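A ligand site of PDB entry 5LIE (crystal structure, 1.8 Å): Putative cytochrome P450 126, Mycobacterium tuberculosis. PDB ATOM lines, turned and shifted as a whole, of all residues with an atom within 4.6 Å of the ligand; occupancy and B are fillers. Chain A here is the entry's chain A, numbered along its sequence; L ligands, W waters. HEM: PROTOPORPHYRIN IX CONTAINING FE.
Water W5 lies within hydrogen-bond range of an oxygen (O2A) of the ligand, the side-chain hydroxyl (OG1) of Thr 83 and the side-chain amide nitrogen (ND2) of Asn 96.
Water W2 lies within hydrogen-bond range of an oxygen (O2A) of the ligand (2.8 Å), the backbone carbonyl oxygen of Asn 96 (2.8 Å), the guanidinium group of Arg 305 (3.3 Å) and a ring nitrogen (ND1) of His 361 (3.3 Å).
Water W4 lies within hydrogen-bond range of the side-chain carboxylate of Glu 328 (3.0 Å) and an oxygen (O1A) of the ligand (3.3 Å).
SG of Cys 363 binds FE of the ligand (2.4 Å).
A ring nitrogen (ND1) of His 361 sits at hydrogen-bond distance from an oxygen (O2D) of the ligand.
An oxygen (O1A) of the ligand is in salt-bridge range of the guanidinium group (NH2) of Arg 305, 2.8 Å away.
O1D of the ligand is in salt-bridge range of NH1 of Arg 107 (2.8 Å).
Leu 95 touches the ligand.
CA of Asn 96 touches O2D of the ligand (3.2 Å).
His 103 touches the ligand (CE1 to O1D, 2.8 Å).
CE of Met 157 touches CMC of the ligand (3.5 Å).
Leu 249 touches the ligand (CD2 to CMD, 3.8 Å).
Ala 253 touches the ligand.
Thr 257 touches the ligand.
OG1 of Thr 258 touches CAB of the ligand, 3.6 Å away.
OG of Ser 261 touches CBB of the ligand, 3.7 Å away.
CG of Pro 299 touches CMB of the ligand, at 3.9 Å.
CD of Lys 303 touches O2A of the ligand, 3.6 Å away.
OE2 of Glu 328 touches CMA of the ligand (3.9 Å).
O of Gly 355 touches CMB of the ligand (3.2 Å).
Phe 356 touches the ligand.
N of Gly 357 touches CMA of the ligand, 3.5 Å away.
Leu 364 touches the ligand.
CA of Gly 365 touches C3C of the ligand, at 3.5 Å.
CB of Ala 369 touches CAB of the ligand, at 3.6 Å.
Hydrophobic or aromatic side chains that line the ligand: Leu 95, His 103, Met 157, Leu 249, Ala 253, Pro 299, Phe 356, His 361 and Ala 369.
Along chain A the residues within 4 Å of the ligand span positions 95 to 369.
The nearest printed residue that does not touch the ligand is Leu 250 (4.01 Å).
SG of Cys 363 lies close to N of Gly 365 (3.3 Å).
O of Phe 356 is in hydrogen-bond range of N of Cys 363.
ND1 of His 103 sits at hydrogen-bond distance from O of Leu 95 (3.4 Å).
The backbone carbonyl oxygen of Val 360 lies close to the guanidinium group of Arg 107.
N of Thr 258 is in hydrogen-bond range of O of Ala 253 (2.9 Å).
O of Thr 258 sits at hydrogen-bond distance from OG of Ser 261 (2.9 Å).
The side-chain carboxylate (OE2) of Glu 328 lies within salt-bridge range of the side-chain amino group (NZ) of Lys 303 (2.6 Å).
NZ of Lys 303 sits at hydrogen-bond distance from OG of Ser 300.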
ATOM      1  N   LEU A  64     -21.494  12.248 -16.257  1.00  0.00           N
ATOM      2  CA  LEU A  64     -21.229  13.157 -17.333  1.00  0.00           C
ATOM      3  C   LEU A  64     -19.762  13.181 -17.674  1.00  0.00           C
ATOM      4  O   LEU A  64     -19.425  13.370 -18.844  1.00  0.00           O
ATOM      5  CB  LEU A  64     -21.731  14.584 -16.996  1.00  0.00           C
ATOM      6  CG  LEU A  64     -23.257  14.660 -16.863  1.00  0.00           C
ATOM      7  CD1 LEU A  64     -23.612  16.095 -16.411  1.00  0.00           C
ATOM      8  CD2 LEU A  64     -23.993  14.347 -18.198  1.00  0.00           C
ATOM      9  N   THR A  83     -29.585   9.590 -26.073  1.00  0.00           N
ATOM     10  CA  THR A  83     -29.587  10.297 -24.801  1.00  0.00           C
ATOM     11  C   THR A  83     -30.967  10.632 -24.276  1.00  0.00           C
ATOM     12  O   THR A  83     -31.083  11.429 -23.390  1.00  0.00           O
ATOM     13  CB  THR A  83     -28.740  11.572 -24.845  1.00  0.00           C
ATOM     14  OG1 THR A  83     -29.257  12.453 -25.834  1.00  0.00           O
ATOM     15  CG2 THR A  83     -27.276  11.230 -25.172  1.00  0.00           C
ATOM     16  N   LEU A  95     -24.780  15.026 -33.169  1.00  0.00           N
ATOM     17  CA  LEU A  95     -23.672  15.342 -32.309  1.00  0.00           C
ATOM     18  C   LEU A  95     -23.902  14.921 -30.843  1.00  0.00           C
ATOM     19  O   LEU A  95     -22.990  14.382 -30.193  1.00  0.00           O
ATOM     20  CB  LEU A  95     -23.408  16.882 -32.375  1.00  0.00           C
ATOM     21  CG  LEU A  95     -22.310  17.385 -31.536  1.00  0.00           C
ATOM     22  CD1 LEU A  95     -21.031  16.695 -32.130  1.00  0.00           C
ATOM     23  CD2 LEU A  95     -22.147  18.910 -31.551  1.00  0.00           C
ATOM     24  N   ASN A  96     -25.076  15.231 -30.289  1.00  0.00           N
ATOM     25  CA  ASN A  96     -25.271  14.973 -28.852  1.00  0.00           C
ATOM     26  C   ASN A  96     -25.542  13.494 -28.581  1.00  0.00           C
ATOM     27  O   ASN A  96     -25.615  13.078 -27.440  1.00  0.00           O
ATOM     28  CB  ASN A  96     -26.388  15.826 -28.250  1.00  0.00           C
ATOM     29  CG  ASN A  96     -27.692  15.571 -28.898  1.00  0.00           C
ATOM     30  OD1 ASN A  96     -27.789  15.528 -30.136  1.00  0.00           O
ATOM     31  ND2 ASN A  96     -28.730  15.385 -28.095  1.00  0.00           N
ATOM     32  N   HIS A 103     -17.500  11.949 -32.562  1.00  0.00           N
ATOM     33  CA  HIS A 103     -17.984  13.102 -31.783  1.00  0.00           C
ATOM     34  C   HIS A 103     -16.962  14.268 -31.801  1.00  0.00           C
ATOM     35  O   HIS A 103     -17.318  15.419 -32.039  1.00  0.00           O
ATOM     36  CB  HIS A 103     -18.275  12.703 -30.349  1.00  0.00           C
ATOM     37  CG  HIS A 103     -18.548  13.877 -29.448  1.00  0.00           C
ATOM     38  ND1 HIS A 103     -19.662  14.686 -29.581  1.00  0.00           N
ATOM     39  CD2 HIS A 103     -17.839  14.359 -28.413  1.00  0.00           C
ATOM     40  CE1 HIS A 103     -19.597  15.651 -28.662  1.00  0.00           C
ATOM     41  NE2 HIS A 103     -18.519  15.458 -27.928  1.00  0.00           N
ATOM     42  N   ARG A 107     -17.873  17.853 -33.343  1.00  0.00           N
ATOM     43  CA  ARG A 107     -18.009  18.946 -32.391  1.00  0.00           C
ATOM     44  C   ARG A 107     -17.105  20.103 -32.780  1.00  0.00           C
ATOM     45  O   ARG A 107     -17.508  21.268 -32.705  1.00  0.00           O
ATOM     46  CB  ARG A 107     -17.733  18.482 -30.959  1.00  0.00           C
ATOM     47  CG  ARG A 107     -17.859  19.588 -29.904  1.00  0.00           C
ATOM     48  CD  ARG A 107     -17.705  18.986 -28.514  1.00  0.00           C
ATOM     49  NE  ARG A 107     -17.462  19.943 -27.440  1.00  0.00           N
ATOM     50  CZ  ARG A 107     -18.417  20.408 -26.637  1.00  0.00           C
ATOM     51  NH1 ARG A 107     -19.704  20.061 -26.865  1.00  0.00           N
ATOM     52  NH2 ARG A 107     -18.079  21.247 -25.664  1.00  0.00           N
ATOM     53  N   MET A 157     -32.497  34.203 -32.957  1.00  0.00           N
ATOM     54  CA  MET A 157     -31.082  33.847 -32.814  1.00  0.00           C
ATOM     55  C   MET A 157     -30.732  32.622 -33.633  1.00  0.00           C
ATOM     56  O   MET A 157     -29.730  32.599 -34.335  1.00  0.00           O
ATOM     57  CB  MET A 157     -30.773  33.501 -31.337  1.00  0.00           C
ATOM     58  CG  MET A 157     -29.421  32.801 -31.191  1.00  0.00           C
ATOM     59  SD  MET A 157     -29.083  32.365 -29.443  1.00  0.00           S
ATOM     60  CE  MET A 157     -30.424  31.132 -29.146  1.00  0.00           C
ATOM     61  N   LEU A 161     -28.076  31.896 -36.743  1.00  0.00           N
ATOM     62  CA  LEU A 161     -27.033  30.854 -36.746  1.00  0.00           C
ATOM     63  C   LEU A 161     -27.160  29.890 -37.924  1.00  0.00           C
ATOM     64  O   LEU A 161     -26.162  29.445 -38.514  1.00  0.00           O
ATOM     65  CB  LEU A 161     -27.106  29.999 -35.476  1.00  0.00           C
ATOM     66  CG  LEU A 161     -26.881  30.664 -34.142  1.00  0.00           C
ATOM     67  CD1 LEU A 161     -27.015  29.591 -32.994  1.00  0.00           C
ATOM     68  CD2 LEU A 161     -25.508  31.351 -34.046  1.00  0.00           C
ATOM     69  N   LEU A 249     -31.514  19.953 -33.705  1.00  0.00           N
ATOM     70  CA  LEU A 249     -30.844  20.144 -32.404  1.00  0.00           C
ATOM     71  C   LEU A 249     -30.755  21.636 -32.124  1.00  0.00           C
ATOM     72  O   LEU A 249     -31.058  22.088 -31.013  1.00  0.00           O
ATOM     73  CB  LEU A 249     -29.426  19.533 -32.426  1.00  0.00           C
ATOM     74  CG  LEU A 249     -28.589  19.699 -31.127  1.00  0.00           C
ATOM     75  CD1 LEU A 249     -29.314  19.043 -29.898  1.00  0.00           C
ATOM     76  CD2 LEU A 249     -27.206  19.081 -31.357  1.00  0.00           C
ATOM     77  N   LEU A 250     -30.249  22.404 -33.084  1.00  0.00           N
ATOM     78  CA  LEU A 250     -30.098  23.870 -32.828  1.00  0.00           C
ATOM     79  C   LEU A 250     -31.441  24.551 -32.700  1.00  0.00           C
ATOM     80  O   LEU A 250     -31.621  25.437 -31.859  1.00  0.00           O
ATOM     81  CB  LEU A 250     -29.314  24.534 -33.922  1.00  0.00           C
ATOM     82  CG  LEU A 250     -27.844  24.790 -33.600  1.00  0.00           C
ATOM     83  CD1 LEU A 250     -27.192  23.586 -33.029  1.00  0.00           C
ATOM     84  CD2 LEU A 250     -27.112  25.272 -34.878  1.00  0.00           C
ATOM     85  N   ALA A 253     -32.738  23.934 -29.400  1.00  0.00           N
ATOM     86  CA  ALA A 253     -31.979  24.597 -28.348  1.00  0.00           C
ATOM     87  C   ALA A 253     -32.437  26.095 -28.187  1.00  0.00           C
ATOM     88  O   ALA A 253     -32.521  26.626 -27.090  1.00  0.00           O
ATOM     89  CB  ALA A 253     -30.486  24.511 -28.668  1.00  0.00           C
ATOM     90  N   THR A 257     -35.285  25.386 -25.544  1.00  0.00           N
ATOM     91  CA  THR A 257     -34.585  25.426 -24.275  1.00  0.00           C
ATOM     92  C   THR A 257     -34.276  26.848 -23.809  1.00  0.00           C
ATOM     93  O   THR A 257     -34.454  27.189 -22.621  1.00  0.00           O
ATOM     94  CB  THR A 257     -33.259  24.588 -24.372  1.00  0.00           C
ATOM     95  OG1 THR A 257     -33.593  23.291 -24.897  1.00  0.00           O
ATOM     96  CG2 THR A 257     -32.697  24.401 -23.028  1.00  0.00           C
ATOM     97  N   THR A 258     -33.789  27.675 -24.718  1.00  0.00           N
ATOM     98  CA  THR A 258     -33.437  29.050 -24.328  1.00  0.00           C
ATOM     99  C   THR A 258     -34.724  29.839 -23.969  1.00  0.00           C
ATOM    100  O   THR A 258     -34.754  30.581 -23.001  1.00  0.00           O
ATOM    101  CB  THR A 258     -32.691  29.734 -25.439  1.00  0.00           C
ATOM    102  OG1 THR A 258     -31.503  28.975 -25.731  1.00  0.00           O
ATOM    103  CG2 THR A 258     -32.252  31.155 -25.006  1.00  0.00           C
ATOM    104  N   SER A 261     -35.573  29.035 -20.449  1.00  0.00           N
ATOM    105  CA  SER A 261     -34.814  29.702 -19.410  1.00  0.00           C
ATOM    106  C   SER A 261     -35.280  31.184 -19.240  1.00  0.00           C
ATOM    107  O   SER A 261     -35.249  31.716 -18.138  1.00  0.00           O
ATOM    108  CB  SER A 261     -33.276  29.738 -19.690  1.00  0.00           C
ATOM    109  OG  SER A 261     -32.941  30.632 -20.784  1.00  0.00           O
ATOM    110  N   PRO A 299     -33.473  24.003 -17.635  1.00  0.00           N
ATOM    111  CA  PRO A 299     -34.489  23.749 -18.695  1.00  0.00           C
ATOM    112  C   PRO A 299     -34.341  22.419 -19.372  1.00  0.00           C
ATOM    113  O   PRO A 299     -35.283  21.912 -19.995  1.00  0.00           O
ATOM    114  CB  PRO A 299     -34.203  24.862 -19.730  1.00  0.00           C
ATOM    115  CG  PRO A 299     -33.347  25.877 -18.987  1.00  0.00           C
ATOM    116  CD  PRO A 299     -32.693  25.215 -17.834  1.00  0.00           C
ATOM    117  N   SER A 300     -33.149  21.806 -19.238  1.00  0.00           N
ATOM    118  CA  SER A 300     -32.938  20.471 -19.779  1.00  0.00           C
ATOM    119  C   SER A 300     -32.596  19.546 -18.602  1.00  0.00           C
ATOM    120  O   SER A 300     -31.439  19.329 -18.311  1.00  0.00           O
ATOM    121  CB  SER A 300     -31.743  20.581 -20.786  1.00  0.00           C
ATOM    122  OG  SER A 300     -31.453  19.337 -21.410  1.00  0.00           O
ATOM    123  N   LYS A 303     -30.903  13.478 -18.646  1.00  0.00           N
ATOM    124  CA  LYS A 303     -30.191  12.978 -19.812  1.00  0.00           C
ATOM    125  C   LYS A 303     -30.078  11.494 -19.603  1.00  0.00           C
ATOM    126  O   LYS A 303     -29.887  11.070 -18.493  1.00  0.00           O
ATOM    127  CB  LYS A 303     -28.700  13.426 -19.847  1.00  0.00           C
ATOM    128  CG  LYS A 303     -28.526  14.897 -19.981  1.00  0.00           C
ATOM    129  CD  LYS A 303     -28.929  15.305 -21.393  1.00  0.00           C
ATOM    130  CE  LYS A 303     -29.153  16.858 -21.444  1.00  0.00           C
ATOM    131  NZ  LYS A 303     -29.983  17.344 -20.334  1.00  0.00           N
ATOM    132  N   ARG A 305     -27.828   7.919 -20.681  1.00  0.00           N
ATOM    133  CA  ARG A 305     -26.610   7.366 -21.249  1.00  0.00           C
ATOM    134  C   ARG A 305     -26.806   5.812 -21.201  1.00  0.00           C
ATOM    135  O   ARG A 305     -27.778   5.310 -20.628  1.00  0.00           O
ATOM    136  CB  ARG A 305     -25.404   7.726 -20.338  1.00  0.00           C
ATOM    137  CG  ARG A 305     -25.153   9.249 -20.215  1.00  0.00           C
ATOM    138  CD  ARG A 305     -24.575   9.810 -21.492  1.00  0.00           C
ATOM    139  NE  ARG A 305     -23.945  11.144 -21.372  1.00  0.00           N
ATOM    140  CZ  ARG A 305     -24.488  12.303 -21.750  1.00  0.00           C
ATOM    141  NH1 ARG A 305     -25.796  12.382 -22.129  1.00  0.00           N
ATOM    142  NH2 ARG A 305     -23.749  13.430 -21.635  1.00  0.00           N
ATOM    143  N   GLU A 328     -30.090  16.375 -13.995  1.00  0.00           N
ATOM    144  CA  GLU A 328     -29.463  17.635 -13.645  1.00  0.00           C
ATOM    145  C   GLU A 328     -30.450  18.570 -12.916  1.00  0.00           C
ATOM    146  O   GLU A 328     -30.070  19.375 -12.067  1.00  0.00           O
ATOM    147  CB  GLU A 328     -28.941  18.380 -14.871  1.00  0.00           C
ATOM    148  CG  GLU A 328     -28.019  17.527 -15.776  1.00  0.00           C
ATOM    149  CD  GLU A 328     -28.827  17.007 -16.965  1.00  0.00           C
ATOM    150  OE1 GLU A 328     -29.736  16.147 -16.706  1.00  0.00           O
ATOM    151  OE2 GLU A 328     -28.602  17.486 -18.137  1.00  0.00           O
ATOM    152  N   GLY A 355     -26.529  22.888 -15.379  1.00  0.00           N
ATOM    153  CA  GLY A 355     -27.605  23.214 -16.320  1.00  0.00           C
ATOM    154  C   GLY A 355     -27.205  23.277 -17.777  1.00  0.00           C
ATOM    155  O   GLY A 355     -28.040  23.178 -18.688  1.00  0.00           O
ATOM    156  N   PHE A 356     -25.883  23.453 -18.013  1.00  0.00           N
ATOM    157  CA  PHE A 356     -25.367  23.360 -19.374  1.00  0.00           C
ATOM    158  C   PHE A 356     -24.555  22.068 -19.609  1.00  0.00           C
ATOM    159  O   PHE A 356     -23.835  21.973 -20.592  1.00  0.00           O
ATOM    160  CB  PHE A 356     -24.396  24.520 -19.630  1.00  0.00           C
ATOM    161  CG  PHE A 356     -25.099  25.889 -19.830  1.00  0.00           C
ATOM    162  CD1 PHE A 356     -26.135  26.019 -20.746  1.00  0.00           C
ATOM    163  CD2 PHE A 356     -24.737  26.986 -19.039  1.00  0.00           C
ATOM    164  CE1 PHE A 356     -26.792  27.284 -20.968  1.00  0.00           C
ATOM    165  CE2 PHE A 356     -25.370  28.268 -19.230  1.00  0.00           C
ATOM    166  CZ  PHE A 356     -26.371  28.397 -20.213  1.00  0.00           C
ATOM    167  N   GLY A 357     -24.678  21.115 -18.711  1.00  0.00           N
ATOM    168  CA  GLY A 357     -23.968  19.854 -18.833  1.00  0.00           C
ATOM    169  C   GLY A 357     -22.555  19.984 -18.243  1.00  0.00           C
ATOM    170  O   GLY A 357     -22.252  20.900 -17.454  1.00  0.00           O
ATOM    171  N   VAL A 360     -17.403  16.274 -22.129  1.00  0.00           N
ATOM    172  CA  VAL A 360     -17.102  16.422 -23.551  1.00  0.00           C
ATOM    173  C   VAL A 360     -18.281  16.915 -24.395  1.00  0.00           C
ATOM    174  O   VAL A 360     -18.068  17.439 -25.490  1.00  0.00           O
ATOM    175  CB  VAL A 360     -16.517  15.148 -24.152  1.00  0.00           C
ATOM    176  CG1 VAL A 360     -15.282  14.777 -23.350  1.00  0.00           C
ATOM    177  CG2 VAL A 360     -17.559  14.024 -24.187  1.00  0.00           C
ATOM    178  N   HIS A 361     -19.510  16.786 -23.851  1.00  0.00           N
ATOM    179  CA  HIS A 361     -20.724  17.245 -24.581  1.00  0.00           C
ATOM    180  C   HIS A 361     -21.223  18.572 -24.040  1.00  0.00           C
ATOM    181  O   HIS A 361     -22.364  18.956 -24.342  1.00  0.00           O
ATOM    182  CB  HIS A 361     -21.868  16.171 -24.488  1.00  0.00           C
ATOM    183  CG  HIS A 361     -21.604  14.930 -25.294  1.00  0.00           C
ATOM    184  ND1 HIS A 361     -21.923  14.836 -26.628  1.00  0.00           N
ATOM    185  CD2 HIS A 361     -21.082  13.716 -24.944  1.00  0.00           C
ATOM    186  CE1 HIS A 361     -21.596  13.637 -27.090  1.00  0.00           C
ATOM    187  NE2 HIS A 361     -21.084  12.939 -26.077  1.00  0.00           N
ATOM    188  N   TYR A 362     -20.390  19.251 -23.220  1.00  0.00           N
ATOM    189  CA  TYR A 362     -20.830  20.516 -22.609  1.00  0.00           C
ATOM    190  C   TYR A 362     -21.455  21.448 -23.659  1.00  0.00           C
ATOM    191  O   TYR A 362     -20.988  21.586 -24.776  1.00  0.00           O
ATOM    192  CB  TYR A 362     -19.655  21.182 -21.879  1.00  0.00           C
ATOM    193  CG  TYR A 362     -20.069  22.488 -21.237  1.00  0.00           C
ATOM    194  CD1 TYR A 362     -20.510  22.494 -19.913  1.00  0.00           C
ATOM    195  CD2 TYR A 362     -19.967  23.720 -21.940  1.00  0.00           C
ATOM    196  CE1 TYR A 362     -20.910  23.697 -19.271  1.00  0.00           C
ATOM    197  CE2 TYR A 362     -20.351  24.916 -21.322  1.00  0.00           C
ATOM    198  CZ  TYR A 362     -20.804  24.878 -20.001  1.00  0.00           C
ATOM    199  OH  TYR A 362     -21.142  26.044 -19.355  1.00  0.00           O
ATOM    200  N   CYS A 363     -22.565  22.065 -23.274  1.00  0.00           N
ATOM    201  CA  CYS A 363     -23.331  22.891 -24.226  1.00  0.00           C
ATOM    202  C   CYS A 363     -22.540  23.873 -25.071  1.00  0.00           C
ATOM    203  O   CYS A 363     -21.847  24.714 -24.522  1.00  0.00           O
ATOM    204  CB  CYS A 363     -24.336  23.653 -23.404  1.00  0.00           C
ATOM    205  SG  CYS A 363     -25.399  24.715 -24.498  1.00  0.00           S
ATOM    206  N   LEU A 364     -22.573  23.713 -26.389  1.00  0.00           N
ATOM    207  CA  LEU A 364     -21.811  24.645 -27.262  1.00  0.00           C
ATOM    208  C   LEU A 364     -22.444  26.026 -27.333  1.00  0.00           C
ATOM    209  O   LEU A 364     -21.763  26.971 -27.736  1.00  0.00           O
ATOM    210  CB  LEU A 364     -21.742  24.118 -28.691  1.00  0.00           C
ATOM    211  CG  LEU A 364     -20.796  22.918 -28.871  1.00  0.00           C
ATOM    212  CD1 LEU A 364     -20.796  22.473 -30.363  1.00  0.00           C
ATOM    213  CD2 LEU A 364     -19.401  23.321 -28.421  1.00  0.00           C
ATOM    214  N   GLY A 365     -23.708  26.134 -26.920  1.00  0.00           N
ATOM    215  CA  GLY A 365     -24.395  27.421 -26.961  1.00  0.00           C
ATOM    216  C   GLY A 365     -24.457  28.142 -25.617  1.00  0.00           C
ATOM    217  O   GLY A 365     -25.240  29.078 -25.484  1.00  0.00           O
ATOM    218  N   LEU A 368     -24.083  31.855 -25.842  1.00  0.00           N
ATOM    219  CA  LEU A 368     -25.200  32.465 -26.594  1.00  0.00           C
ATOM    220  C   LEU A 368     -26.437  32.530 -25.705  1.00  0.00           C
ATOM    221  O   LEU A 368     -27.205  33.497 -25.733  1.00  0.00           O
ATOM    222  CB  LEU A 368     -25.496  31.654 -27.828  1.00  0.00           C
ATOM    223  CG  LEU A 368     -24.626  31.769 -29.050  1.00  0.00           C
ATOM    224  CD1 LEU A 368     -24.962  30.697 -30.051  1.00  0.00           C
ATOM    225  CD2 LEU A 368     -24.902  33.192 -29.674  1.00  0.00           C
ATOM    226  N   ALA A 369     -26.677  31.488 -24.913  1.00  0.00           N
ATOM    227  CA  ALA A 369     -27.861  31.525 -24.031  1.00  0.00           C
ATOM    228  C   ALA A 369     -27.710  32.595 -22.978  1.00  0.00           C
ATOM    229  O   ALA A 369     -28.650  33.291 -22.625  1.00  0.00           O
ATOM    230  CB  ALA A 369     -28.091  30.122 -23.299  1.00  0.00           C
HETATM  231  CHA HEM L   1     -25.572  20.402 -25.407  1.00  0.00           C
HETATM  232  CHB HEM L   1     -28.351  22.782 -22.163  1.00  0.00           C
HETATM  233  CHC HEM L   1     -28.852  26.477 -25.251  1.00  0.00           C
HETATM  234  CHD HEM L   1     -26.273  24.046 -28.598  1.00  0.00           C
HETATM  235  C1A HEM L   1     -26.229  20.743 -24.246  1.00  0.00           C
HETATM  236  C2A HEM L   1     -26.298  19.938 -23.041  1.00  0.00           C
HETATM  237  C3A HEM L   1     -27.093  20.585 -22.170  1.00  0.00           C
HETATM  238  C4A HEM L   1     -27.532  21.842 -22.787  1.00  0.00           C
HETATM  239  CMA HEM L   1     -27.411  20.180 -20.747  1.00  0.00           C
HETATM  240  CAA HEM L   1     -25.541  18.575 -22.806  1.00  0.00           C
HETATM  241  CBA HEM L   1     -26.188  17.413 -23.543  1.00  0.00           C
HETATM  242  CGA HEM L   1     -25.653  16.064 -23.025  1.00  0.00           C
HETATM  243  O1A HEM L   1     -24.869  16.001 -22.049  1.00  0.00           O
HETATM  244  O2A HEM L   1     -26.066  15.045 -23.593  1.00  0.00           O
HETATM  245  C1B HEM L   1     -28.721  23.983 -22.738  1.00  0.00           C
HETATM  246  C2B HEM L   1     -29.474  25.035 -22.054  1.00  0.00           C
HETATM  247  C3B HEM L   1     -29.637  26.038 -22.907  1.00  0.00           C
HETATM  248  C4B HEM L   1     -28.940  25.663 -24.147  1.00  0.00           C
HETATM  249  CMB HEM L   1     -30.002  24.882 -20.620  1.00  0.00           C
HETATM  250  CAB HEM L   1     -30.329  27.404 -22.729  1.00  0.00           C
HETATM  251  CBB HEM L   1     -30.446  27.965 -21.508  1.00  0.00           C
HETATM  252  C1C HEM L   1     -28.141  26.169 -26.397  1.00  0.00           C
HETATM  253  C2C HEM L   1     -28.032  26.999 -27.570  1.00  0.00           C
HETATM  254  C3C HEM L   1     -27.296  26.316 -28.486  1.00  0.00           C
HETATM  255  C4C HEM L   1     -26.967  25.022 -27.940  1.00  0.00           C
HETATM  256  CMC HEM L   1     -28.562  28.459 -27.751  1.00  0.00           C
HETATM  257  CAC HEM L   1     -26.899  26.836 -29.854  1.00  0.00           C
HETATM  258  CBC HEM L   1     -25.637  26.645 -30.292  1.00  0.00           C
HETATM  259  C1D HEM L   1     -25.930  22.825 -28.062  1.00  0.00           C
HETATM  260  C2D HEM L   1     -25.243  21.813 -28.795  1.00  0.00           C
HETATM  261  C3D HEM L   1     -25.024  20.688 -27.826  1.00  0.00           C
HETATM  262  C4D HEM L   1     -25.590  21.136 -26.568  1.00  0.00           C
HETATM  263  CMD HEM L   1     -24.854  21.842 -30.281  1.00  0.00           C
HETATM  264  CAD HEM L   1     -24.341  19.324 -28.148  1.00  0.00           C
HETATM  265  CBD HEM L   1     -22.879  19.411 -27.693  1.00  0.00           C
HETATM  266  CGD HEM L   1     -22.278  18.041 -27.860  1.00  0.00           C
HETATM  267  O1D HEM L   1     -21.082  17.905 -28.106  1.00  0.00           O
HETATM  268  O2D HEM L   1     -23.051  17.058 -27.793  1.00  0.00           O
HETATM  269  NA  HEM L   1     -27.002  21.879 -24.045  1.00  0.00           N
HETATM  270  NB  HEM L   1     -28.430  24.394 -23.986  1.00  0.00           N
HETATM  271  NC  HEM L   1     -27.494  24.988 -26.673  1.00  0.00           N
HETATM  272  ND  HEM L   1     -26.114  22.408 -26.760  1.00  0.00           N
HETATM  273 FE   HEM L   1     -27.227  23.430 -25.360  1.00  0.00          FE
HETATM  274  O   HOH W   1     -22.729  17.438 -20.913  1.00  0.00           O
HETATM  275  O   HOH W   2     -24.392  13.342 -24.977  1.00  0.00           O
HETATM  276  O   HOH W   3     -29.890  19.688 -23.930  1.00  0.00           O
HETATM  277  O   HOH W   4     -25.839  17.305 -19.167  1.00  0.00           O
HETATM  278  O   HOH W   5     -28.131  15.016 -25.230  1.00  0.00           O
